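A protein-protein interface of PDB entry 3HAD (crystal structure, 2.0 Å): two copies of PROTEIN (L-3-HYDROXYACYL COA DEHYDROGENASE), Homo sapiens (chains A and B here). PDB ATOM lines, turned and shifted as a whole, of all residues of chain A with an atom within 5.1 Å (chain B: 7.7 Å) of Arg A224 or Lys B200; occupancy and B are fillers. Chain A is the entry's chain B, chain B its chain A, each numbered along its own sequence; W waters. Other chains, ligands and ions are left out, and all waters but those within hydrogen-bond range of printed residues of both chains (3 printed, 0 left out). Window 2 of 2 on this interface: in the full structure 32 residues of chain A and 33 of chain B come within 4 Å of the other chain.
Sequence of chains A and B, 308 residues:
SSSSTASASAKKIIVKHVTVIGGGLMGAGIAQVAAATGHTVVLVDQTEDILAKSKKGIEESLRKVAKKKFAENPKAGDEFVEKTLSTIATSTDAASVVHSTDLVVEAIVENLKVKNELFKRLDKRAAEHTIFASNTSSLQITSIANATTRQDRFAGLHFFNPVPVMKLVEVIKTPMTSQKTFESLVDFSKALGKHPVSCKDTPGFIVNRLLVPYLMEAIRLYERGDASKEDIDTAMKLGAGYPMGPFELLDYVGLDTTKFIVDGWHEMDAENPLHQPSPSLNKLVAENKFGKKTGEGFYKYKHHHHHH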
ATOM      1  N   ILE A 219      21.748  -7.538  20.862  1.00  0.00           N
ATOM      2  CA  ILE A 219      22.364  -6.549  21.738  1.00  0.00           C
ATOM      3  C   ILE A 219      21.942  -5.145  21.308  1.00  0.00           C
ATOM      4  O   ILE A 219      21.571  -4.315  22.150  1.00  0.00           O
ATOM      5  CB  ILE A 219      23.909  -6.599  21.685  1.00  0.00           C
ATOM      6  CG1 ILE A 219      24.420  -7.967  22.164  1.00  0.00           C
ATOM      7  CG2 ILE A 219      24.474  -5.488  22.558  1.00  0.00           C
ATOM      8  CD1 ILE A 219      25.875  -8.238  21.821  1.00  0.00           C
ATOM      9  N   ARG A 220      22.001  -4.873  20.001  1.00  0.00           N
ATOM     10  CA  ARG A 220      21.623  -3.546  19.509  1.00  0.00           C
ATOM     11  C   ARG A 220      20.172  -3.169  19.831  1.00  0.00           C
ATOM     12  O   ARG A 220      19.890  -2.010  20.142  1.00  0.00           O
ATOM     13  CB  ARG A 220      21.843  -3.426  17.991  1.00  0.00           C
ATOM     14  CG  ARG A 220      23.253  -3.667  17.556  1.00  0.00           C
ATOM     15  CD  ARG A 220      23.503  -3.156  16.154  1.00  0.00           C
ATOM     16  NE  ARG A 220      24.878  -3.432  15.772  1.00  0.00           N
ATOM     17  CZ  ARG A 220      25.296  -4.577  15.243  1.00  0.00           C
ATOM     18  NH1 ARG A 220      24.428  -5.540  14.972  1.00  0.00           N
ATOM     19  NH2 ARG A 220      26.577  -4.736  14.937  1.00  0.00           N
ATOM     20  N   LEU A 221      19.258  -4.133  19.743  1.00  0.00           N
ATOM     21  CA  LEU A 221      17.847  -3.884  20.040  1.00  0.00           C
ATOM     22  C   LEU A 221      17.784  -3.417  21.486  1.00  0.00           C
ATOM     23  O   LEU A 221      17.065  -2.466  21.839  1.00  0.00           O
ATOM     24  CB  LEU A 221      17.033  -5.170  19.904  1.00  0.00           C
ATOM     25  CG  LEU A 221      15.526  -5.013  20.117  1.00  0.00           C
ATOM     26  CD1 LEU A 221      14.900  -4.765  18.762  1.00  0.00           C
ATOM     27  CD2 LEU A 221      14.906  -6.273  20.707  1.00  0.00           C
ATOM     28  N   TYR A 222      18.551  -4.110  22.323  1.00  0.00           N
ATOM     29  CA  TYR A 222      18.626  -3.791  23.740  1.00  0.00           C
ATOM     30  C   TYR A 222      19.221  -2.396  23.935  1.00  0.00           C
ATOM     31  O   TYR A 222      18.635  -1.570  24.631  1.00  0.00           O
ATOM     32  CB  TYR A 222      19.477  -4.849  24.473  1.00  0.00           C
ATOM     33  CG  TYR A 222      19.744  -4.552  25.933  1.00  0.00           C
ATOM     34  CD1 TYR A 222      18.695  -4.395  26.840  1.00  0.00           C
ATOM     35  CD2 TYR A 222      21.054  -4.415  26.407  1.00  0.00           C
ATOM     36  CE1 TYR A 222      18.941  -4.109  28.179  1.00  0.00           C
ATOM     37  CE2 TYR A 222      21.314  -4.129  27.741  1.00  0.00           C
ATOM     38  CZ  TYR A 222      20.257  -3.974  28.623  1.00  0.00           C
ATOM     39  OH  TYR A 222      20.510  -3.673  29.943  1.00  0.00           O
ATOM     40  N   GLU A 223      20.370  -2.136  23.317  1.00  0.00           N
ATOM     41  CA  GLU A 223      21.029  -0.831  23.451  1.00  0.00           C
ATOM     42  C   GLU A 223      20.200   0.325  22.885  1.00  0.00           C
ATOM     43  O   GLU A 223      20.479   1.491  23.164  1.00  0.00           O
ATOM     44  CB  GLU A 223      22.391  -0.821  22.751  1.00  0.00           C
ATOM     45  CG  GLU A 223      23.335  -1.935  23.165  1.00  0.00           C
ATOM     46  CD  GLU A 223      24.742  -1.698  22.665  1.00  0.00           C
ATOM     47  OE1 GLU A 223      25.527  -1.045  23.381  1.00  0.00           O
ATOM     48  OE2 GLU A 223      25.061  -2.140  21.545  1.00  0.00           O
ATOM     49  N   ARG A 224      19.183   0.005  22.100  1.00  0.00           N
ATOM     50  CA  ARG A 224      18.349   1.035  21.504  1.00  0.00           C
ATOM     51  C   ARG A 224      17.277   1.412  22.516  1.00  0.00           C
ATOM     52  O   ARG A 224      16.663   2.478  22.435  1.00  0.00           O
ATOM     53  CB  ARG A 224      17.724   0.467  20.239  1.00  0.00           C
ATOM     54  CG  ARG A 224      17.558   1.434  19.124  1.00  0.00           C
ATOM     55  CD  ARG A 224      17.864   0.706  17.827  1.00  0.00           C
ATOM     56  NE  ARG A 224      17.044  -0.486  17.628  1.00  0.00           N
ATOM     57  CZ  ARG A 224      17.519  -1.580  17.049  1.00  0.00           C
ATOM     58  NH1 ARG A 224      18.774  -1.585  16.650  1.00  0.00           N
ATOM     59  NH2 ARG A 224      16.770  -2.663  16.879  1.00  0.00           N
ATOM     60  N   GLY A 225      17.064   0.519  23.478  1.00  0.00           N
ATOM     61  CA  GLY A 225      16.073   0.746  24.509  1.00  0.00           C
ATOM     62  C   GLY A 225      14.727   0.182  24.107  1.00  0.00           C
ATOM     63  O   GLY A 225      13.721   0.466  24.755  1.00  0.00           O
ATOM     64  N   ASP A 226      14.705  -0.636  23.057  1.00  0.00           N
ATOM     65  CA  ASP A 226      13.448  -1.190  22.563  1.00  0.00           C
ATOM     66  C   ASP A 226      12.811  -2.292  23.402  1.00  0.00           C
ATOM     67  O   ASP A 226      11.592  -2.469  23.369  1.00  0.00           O
ATOM     68  CB  ASP A 226      13.610  -1.668  21.115  1.00  0.00           C
ATOM     69  CG  ASP A 226      14.111  -0.554  20.189  1.00  0.00           C
ATOM     70  OD1 ASP A 226      13.964   0.624  20.569  1.00  0.00           O
ATOM     71  OD2 ASP A 226      14.631  -0.856  19.087  1.00  0.00           O
ATOM     72  N   ILE B 141       1.926   0.468  14.951  1.00  0.00           N
ATOM     73  CA  ILE B 141       0.775   0.557  15.822  1.00  0.00           C
ATOM     74  C   ILE B 141       0.377   2.040  15.902  1.00  0.00           C
ATOM     75  O   ILE B 141      -0.795   2.382  15.817  1.00  0.00           O
ATOM     76  CB  ILE B 141       1.102   0.046  17.236  1.00  0.00           C
ATOM     77  CG1 ILE B 141       1.563  -1.420  17.177  1.00  0.00           C
ATOM     78  CG2 ILE B 141      -0.106   0.207  18.139  1.00  0.00           C
ATOM     79  CD1 ILE B 141       0.618  -2.347  16.447  1.00  0.00           C
ATOM     80  N   THR B 142       1.373   2.911  16.041  1.00  0.00           N
ATOM     81  CA  THR B 142       1.134   4.348  16.144  1.00  0.00           C
ATOM     82  C   THR B 142       0.286   4.865  14.983  1.00  0.00           C
ATOM     83  O   THR B 142      -0.620   5.670  15.182  1.00  0.00           O
ATOM     84  CB  THR B 142       2.470   5.135  16.185  1.00  0.00           C
ATOM     85  OG1 THR B 142       3.250   4.703  17.310  1.00  0.00           O
ATOM     86  CG2 THR B 142       2.212   6.627  16.309  1.00  0.00           C
ATOM     87  N   VAL B 171       3.366  -7.500  23.573  1.00  0.00           N
ATOM     88  CA  VAL B 171       2.459  -6.403  23.910  1.00  0.00           C
ATOM     89  C   VAL B 171       3.164  -5.126  23.459  1.00  0.00           C
ATOM     90  O   VAL B 171       4.149  -4.713  24.067  1.00  0.00           O
ATOM     91  CB  VAL B 171       2.203  -6.369  25.433  1.00  0.00           C
ATOM     92  CG1 VAL B 171       1.255  -5.226  25.789  1.00  0.00           C
ATOM     93  CG2 VAL B 171       1.618  -7.721  25.884  1.00  0.00           C
ATOM     94  N   ILE B 172       2.658  -4.501  22.398  1.00  0.00           N
ATOM     95  CA  ILE B 172       3.304  -3.316  21.848  1.00  0.00           C
ATOM     96  C   ILE B 172       2.717  -1.998  22.316  1.00  0.00           C
ATOM     97  O   ILE B 172       1.540  -1.715  22.112  1.00  0.00           O
ATOM     98  CB  ILE B 172       3.267  -3.350  20.324  1.00  0.00           C
ATOM     99  CG1 ILE B 172       3.746  -4.724  19.840  1.00  0.00           C
ATOM    100  CG2 ILE B 172       4.133  -2.225  19.766  1.00  0.00           C
ATOM    101  CD1 ILE B 172       5.134  -5.104  20.365  1.00  0.00           C
ATOM    102  N   LYS B 173       3.568  -1.176  22.907  1.00  0.00           N
ATOM    103  CA  LYS B 173       3.138   0.102  23.446  1.00  0.00           C
ATOM    104  C   LYS B 173       3.574   1.280  22.578  1.00  0.00           C
ATOM    105  O   LYS B 173       4.740   1.365  22.200  1.00  0.00           O
ATOM    106  CB  LYS B 173       3.725   0.228  24.853  1.00  0.00           C
ATOM    107  CG  LYS B 173       3.134   1.289  25.729  1.00  0.00           C
ATOM    108  CD  LYS B 173       3.648   1.112  27.159  1.00  0.00           C
ATOM    109  CE  LYS B 173       3.019   2.132  28.112  1.00  0.00           C
ATOM    110  NZ  LYS B 173       3.488   1.951  29.531  1.00  0.00           N
ATOM    111  N   THR B 174       2.642   2.177  22.234  1.00  0.00           N
ATOM    112  CA  THR B 174       3.012   3.365  21.453  1.00  0.00           C
ATOM    113  C   THR B 174       3.278   4.424  22.505  1.00  0.00           C
ATOM    114  O   THR B 174       2.988   4.229  23.686  1.00  0.00           O
ATOM    115  CB  THR B 174       1.861   3.940  20.573  1.00  0.00           C
ATOM    116  OG1 THR B 174       0.881   4.551  21.421  1.00  0.00           O
ATOM    117  CG2 THR B 174       1.211   2.865  19.745  1.00  0.00           C
ATOM    118  N   PRO B 175       3.835   5.567  22.097  1.00  0.00           N
ATOM    119  CA  PRO B 175       4.091   6.607  23.087  1.00  0.00           C
ATOM    120  C   PRO B 175       2.806   7.083  23.770  1.00  0.00           C
ATOM    121  O   PRO B 175       2.862   7.717  24.822  1.00  0.00           O
ATOM    122  CB  PRO B 175       4.755   7.703  22.247  1.00  0.00           C
ATOM    123  CG  PRO B 175       5.478   6.883  21.171  1.00  0.00           C
ATOM    124  CD  PRO B 175       4.316   5.999  20.776  1.00  0.00           C
ATOM    125  N   SER B 198       7.278  -7.108  26.458  1.00  0.00           N
ATOM    126  CA  SER B 198       7.069  -5.718  26.077  1.00  0.00           C
ATOM    127  C   SER B 198       8.051  -5.232  25.029  1.00  0.00           C
ATOM    128  O   SER B 198       9.219  -5.593  25.066  1.00  0.00           O
ATOM    129  CB  SER B 198       7.193  -4.849  27.327  1.00  0.00           C
ATOM    130  OG  SER B 198       7.144  -3.472  27.005  1.00  0.00           O
ATOM    131  N   CYS B 199       7.576  -4.421  24.083  1.00  0.00           N
ATOM    132  CA  CYS B 199       8.458  -3.875  23.057  1.00  0.00           C
ATOM    133  C   CYS B 199       7.909  -2.552  22.518  1.00  0.00           C
ATOM    134  O   CYS B 199       6.692  -2.370  22.435  1.00  0.00           O
ATOM    135  CB  CYS B 199       8.643  -4.879  21.912  1.00  0.00           C
ATOM    136  SG  CYS B 199       9.869  -4.355  20.645  1.00  0.00           S
ATOM    137  N   LYS B 200       8.799  -1.617  22.180  1.00  0.00           N
ATOM    138  CA  LYS B 200       8.352  -0.335  21.620  1.00  0.00           C
ATOM    139  C   LYS B 200       7.741  -0.597  20.248  1.00  0.00           C
ATOM    140  O   LYS B 200       7.930  -1.668  19.666  1.00  0.00           O
ATOM    141  CB  LYS B 200       9.518   0.646  21.417  1.00  0.00           C
ATOM    142  CG  LYS B 200      10.124   1.239  22.662  1.00  0.00           C
ATOM    143  CD  LYS B 200      11.205   2.243  22.253  1.00  0.00           C
ATOM    144  CE  LYS B 200      11.966   2.797  23.449  1.00  0.00           C
ATOM    145  NZ  LYS B 200      13.166   3.559  22.986  1.00  0.00           N
ATOM    146  N   ASP B 201       7.021   0.392  19.735  1.00  0.00           N
ATOM    147  CA  ASP B 201       6.399   0.284  18.416  1.00  0.00           C
ATOM    148  C   ASP B 201       7.499   0.496  17.375  1.00  0.00           C
ATOM    149  O   ASP B 201       7.569   1.544  16.722  1.00  0.00           O
ATOM    150  CB  ASP B 201       5.324   1.363  18.241  1.00  0.00           C
ATOM    151  CG  ASP B 201       4.636   1.288  16.889  1.00  0.00           C
ATOM    152  OD1 ASP B 201       4.654   0.204  16.263  1.00  0.00           O
ATOM    153  OD2 ASP B 201       4.060   2.317  16.463  1.00  0.00           O
ATOM    154  N   THR B 202       8.360  -0.500  17.225  1.00  0.00           N
ATOM    155  CA  THR B 202       9.445  -0.419  16.269  1.00  0.00           C
ATOM    156  C   THR B 202       9.259  -1.576  15.294  1.00  0.00           C
ATOM    157  O   THR B 202       8.735  -2.618  15.662  1.00  0.00           O
ATOM    158  CB  THR B 202      10.792  -0.489  16.996  1.00  0.00           C
ATOM    159  OG1 THR B 202      10.871  -1.704  17.746  1.00  0.00           O
ATOM    160  CG2 THR B 202      10.929   0.703  17.962  1.00  0.00           C
ATOM    161  N   PRO B 203       9.650  -1.398  14.026  1.00  0.00           N
ATOM    162  CA  PRO B 203       9.478  -2.477  13.048  1.00  0.00           C
ATOM    163  C   PRO B 203      10.022  -3.848  13.437  1.00  0.00           C
ATOM    164  O   PRO B 203      11.179  -3.993  13.848  1.00  0.00           O
ATOM    165  CB  PRO B 203      10.127  -1.901  11.779  1.00  0.00           C
ATOM    166  CG  PRO B 203      11.101  -0.869  12.327  1.00  0.00           C
ATOM    167  CD  PRO B 203      10.244  -0.218  13.376  1.00  0.00           C
ATOM    168  N   GLY B 204       9.159  -4.851  13.310  1.00  0.00           N
ATOM    169  CA  GLY B 204       9.551  -6.206  13.643  1.00  0.00           C
ATOM    170  C   GLY B 204       9.380  -6.528  15.117  1.00  0.00           C
ATOM    171  O   GLY B 204       9.369  -7.692  15.490  1.00  0.00           O
ATOM    172  N   PHE B 205       9.228  -5.497  15.941  1.00  0.00           N
ATOM    173  CA  PHE B 205       9.063  -5.679  17.381  1.00  0.00           C
ATOM    174  C   PHE B 205      10.286  -6.490  17.848  1.00  0.00           C
ATOM    175  O   PHE B 205      11.420  -6.084  17.605  1.00  0.00           O
ATOM    176  CB  PHE B 205       7.744  -6.421  17.661  1.00  0.00           C
ATOM    177  CG  PHE B 205       6.520  -5.713  17.109  1.00  0.00           C
ATOM    178  CD1 PHE B 205       6.442  -4.316  17.105  1.00  0.00           C
ATOM    179  CD2 PHE B 205       5.456  -6.443  16.592  1.00  0.00           C
ATOM    180  CE1 PHE B 205       5.320  -3.652  16.589  1.00  0.00           C
ATOM    181  CE2 PHE B 205       4.333  -5.795  16.072  1.00  0.00           C
ATOM    182  CZ  PHE B 205       4.265  -4.399  16.071  1.00  0.00           C
ATOM    183  N   ILE B 206      10.084  -7.622  18.507  1.00  0.00           N
ATOM    184  CA  ILE B 206      11.252  -8.394  18.931  1.00  0.00           C
ATOM    185  C   ILE B 206      11.528  -9.584  18.024  1.00  0.00           C
ATOM    186  O   ILE B 206      12.509  -9.600  17.274  1.00  0.00           O
ATOM    187  CB  ILE B 206      11.129  -8.889  20.392  1.00  0.00           C
ATOM    188  CG1 ILE B 206      11.139  -7.685  21.349  1.00  0.00           C
ATOM    189  CG2 ILE B 206      12.287  -9.846  20.691  1.00  0.00           C
ATOM    190  CD1 ILE B 206      10.763  -7.994  22.805  1.00  0.00           C
ATOM    191  N   ARG B 209      11.970  -8.923  14.148  1.00  0.00           N
ATOM    192  CA  ARG B 209      13.133  -8.057  13.953  1.00  0.00           C
ATOM    193  C   ARG B 209      14.455  -8.808  14.093  1.00  0.00           C
ATOM    194  O   ARG B 209      15.460  -8.408  13.502  1.00  0.00           O
ATOM    195  CB  ARG B 209      13.107  -6.892  14.941  1.00  0.00           C
ATOM    196  CG  ARG B 209      14.330  -5.967  14.870  1.00  0.00           C
ATOM    197  CD  ARG B 209      14.430  -5.195  13.528  1.00  0.00           C
ATOM    198  NE  ARG B 209      15.570  -4.265  13.509  1.00  0.00           N
ATOM    199  CZ  ARG B 209      16.843  -4.632  13.356  1.00  0.00           C
ATOM    200  NH1 ARG B 209      17.158  -5.913  13.177  1.00  0.00           N
ATOM    201  NH2 ARG B 209      17.805  -3.713  13.360  1.00  0.00           N
ATOM    202  N   LEU B 210      14.466  -9.886  14.882  1.00  0.00           N
ATOM    203  CA  LEU B 210      15.680 -10.670  15.082  1.00  0.00           C
ATOM    204  C   LEU B 210      15.639 -11.929  14.235  1.00  0.00           C
ATOM    205  O   LEU B 210      16.677 -12.458  13.843  1.00  0.00           O
ATOM    206  CB  LEU B 210      15.840 -11.029  16.573  1.00  0.00           C
ATOM    207  CG  LEU B 210      16.045  -9.785  17.444  1.00  0.00           C
ATOM    208  CD1 LEU B 210      16.183 -10.159  18.928  1.00  0.00           C
ATOM    209  CD2 LEU B 210      17.304  -9.059  16.962  1.00  0.00           C
HETATM  210  O   HOH W   1      13.958  -2.407  17.179  1.00  0.00           O
HETATM  211  O   HOH W   2      20.440  -2.883  14.713  1.00  0.00           O
HETATM  212  O   HOH W   3      18.781  -4.844  16.216  1.00  0.00           O
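Among the printed residues, merely in contact across the chains: Gly A225 with Lys B200, Arg A224 with Lys B200, Arg A224 with Arg B209 and Leu A221 with Phe B205.
No position is printed for both chains.
Of the printed residues of chain B, Leu A221 touches Phe B205.
Of chain B, only Lys B200 (3.7 Å) and Arg B209 (3.8 Å) come within 4 Å of Arg A224.
Thr B174 touches none of the printed residues of chain A.
Lys B200 touches three residues of chain A.
Gly B204 touches none of the printed residues of chain A.
Of the printed residues of chain A, Phe B205 touches Leu A221.
Of the printed residues of chain A, Arg B209 touches Arg A224.
The nearest residue of chain B that does not touch Arg A224 is Thr B202 (6.0 Å).
The nearest printed residue of chain A that does not touch Arg B209 is Leu A221 (4.1 Å).
Hydrophobic or aromatic side chains of chain A that line the printed part of chain B: Leu A221.
Of the 18 printed residues of chain B, 4 touch a printed residue of chain A.
Printed residues of chain B that touch a printed residue of chain A: Cys B199, Lys B200, Phe B205 and Arg B209.
Along chain B the printed residues that touch a printed residue of chain A span positions 199 to 209.
Among the printed residues, Asp or Glu carboxylates within 4 Å of a Lys or Arg side-chain nitrogen of the other chain: Asp A226 with Lys B200.
The backbone carbonyl oxygen of Val B171 is in hydrogen-bond range of the backbone NH of Cys B199 (3.4 Å).
The backbone NH (N) of Lys B173 sits at hydrogen-bond distance from the backbone carbonyl oxygen (O) of Cys B199 (3.4 Å).
The backbone NH of Arg B209 lies within hydrogen-bond range of the backbone carbonyl oxygen of Gly B204.
The backbone carbonyl oxygen (O) of Leu A221 sits at hydrogen-bond distance from the backbone NH (N) of Asp A226.
The guanidinium group of Arg A224 lies within salt-bridge range of the side-chain carboxylate of Asp A226, at 2.8 Å.
The side-chain sulfur of Cys B199 sits close to the backbone carbonyl oxygen of Asp A226 (3.7 Å).
OD1 of Asp A226 lies within salt-bridge range of NZ of Lys B200 (3.9 Å).
Water W1 lies within hydrogen-bond range of OD2 of Asp A226 (2.5 Å), NH2 of Arg A224 (2.8 Å) and OG1 of Thr B202 (3.2 Å).
Water W2 lies within hydrogen-bond range of the guanidinium group of Arg A224 (2.9 Å) and the guanidinium group of Arg B209 (3.1 Å).
Water W3 lies within hydrogen-bond range of the guanidinium group (NH2) of Arg A224 (3.0 Å) and the guanidinium group (NH2) of Arg B209 (3.2 Å).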
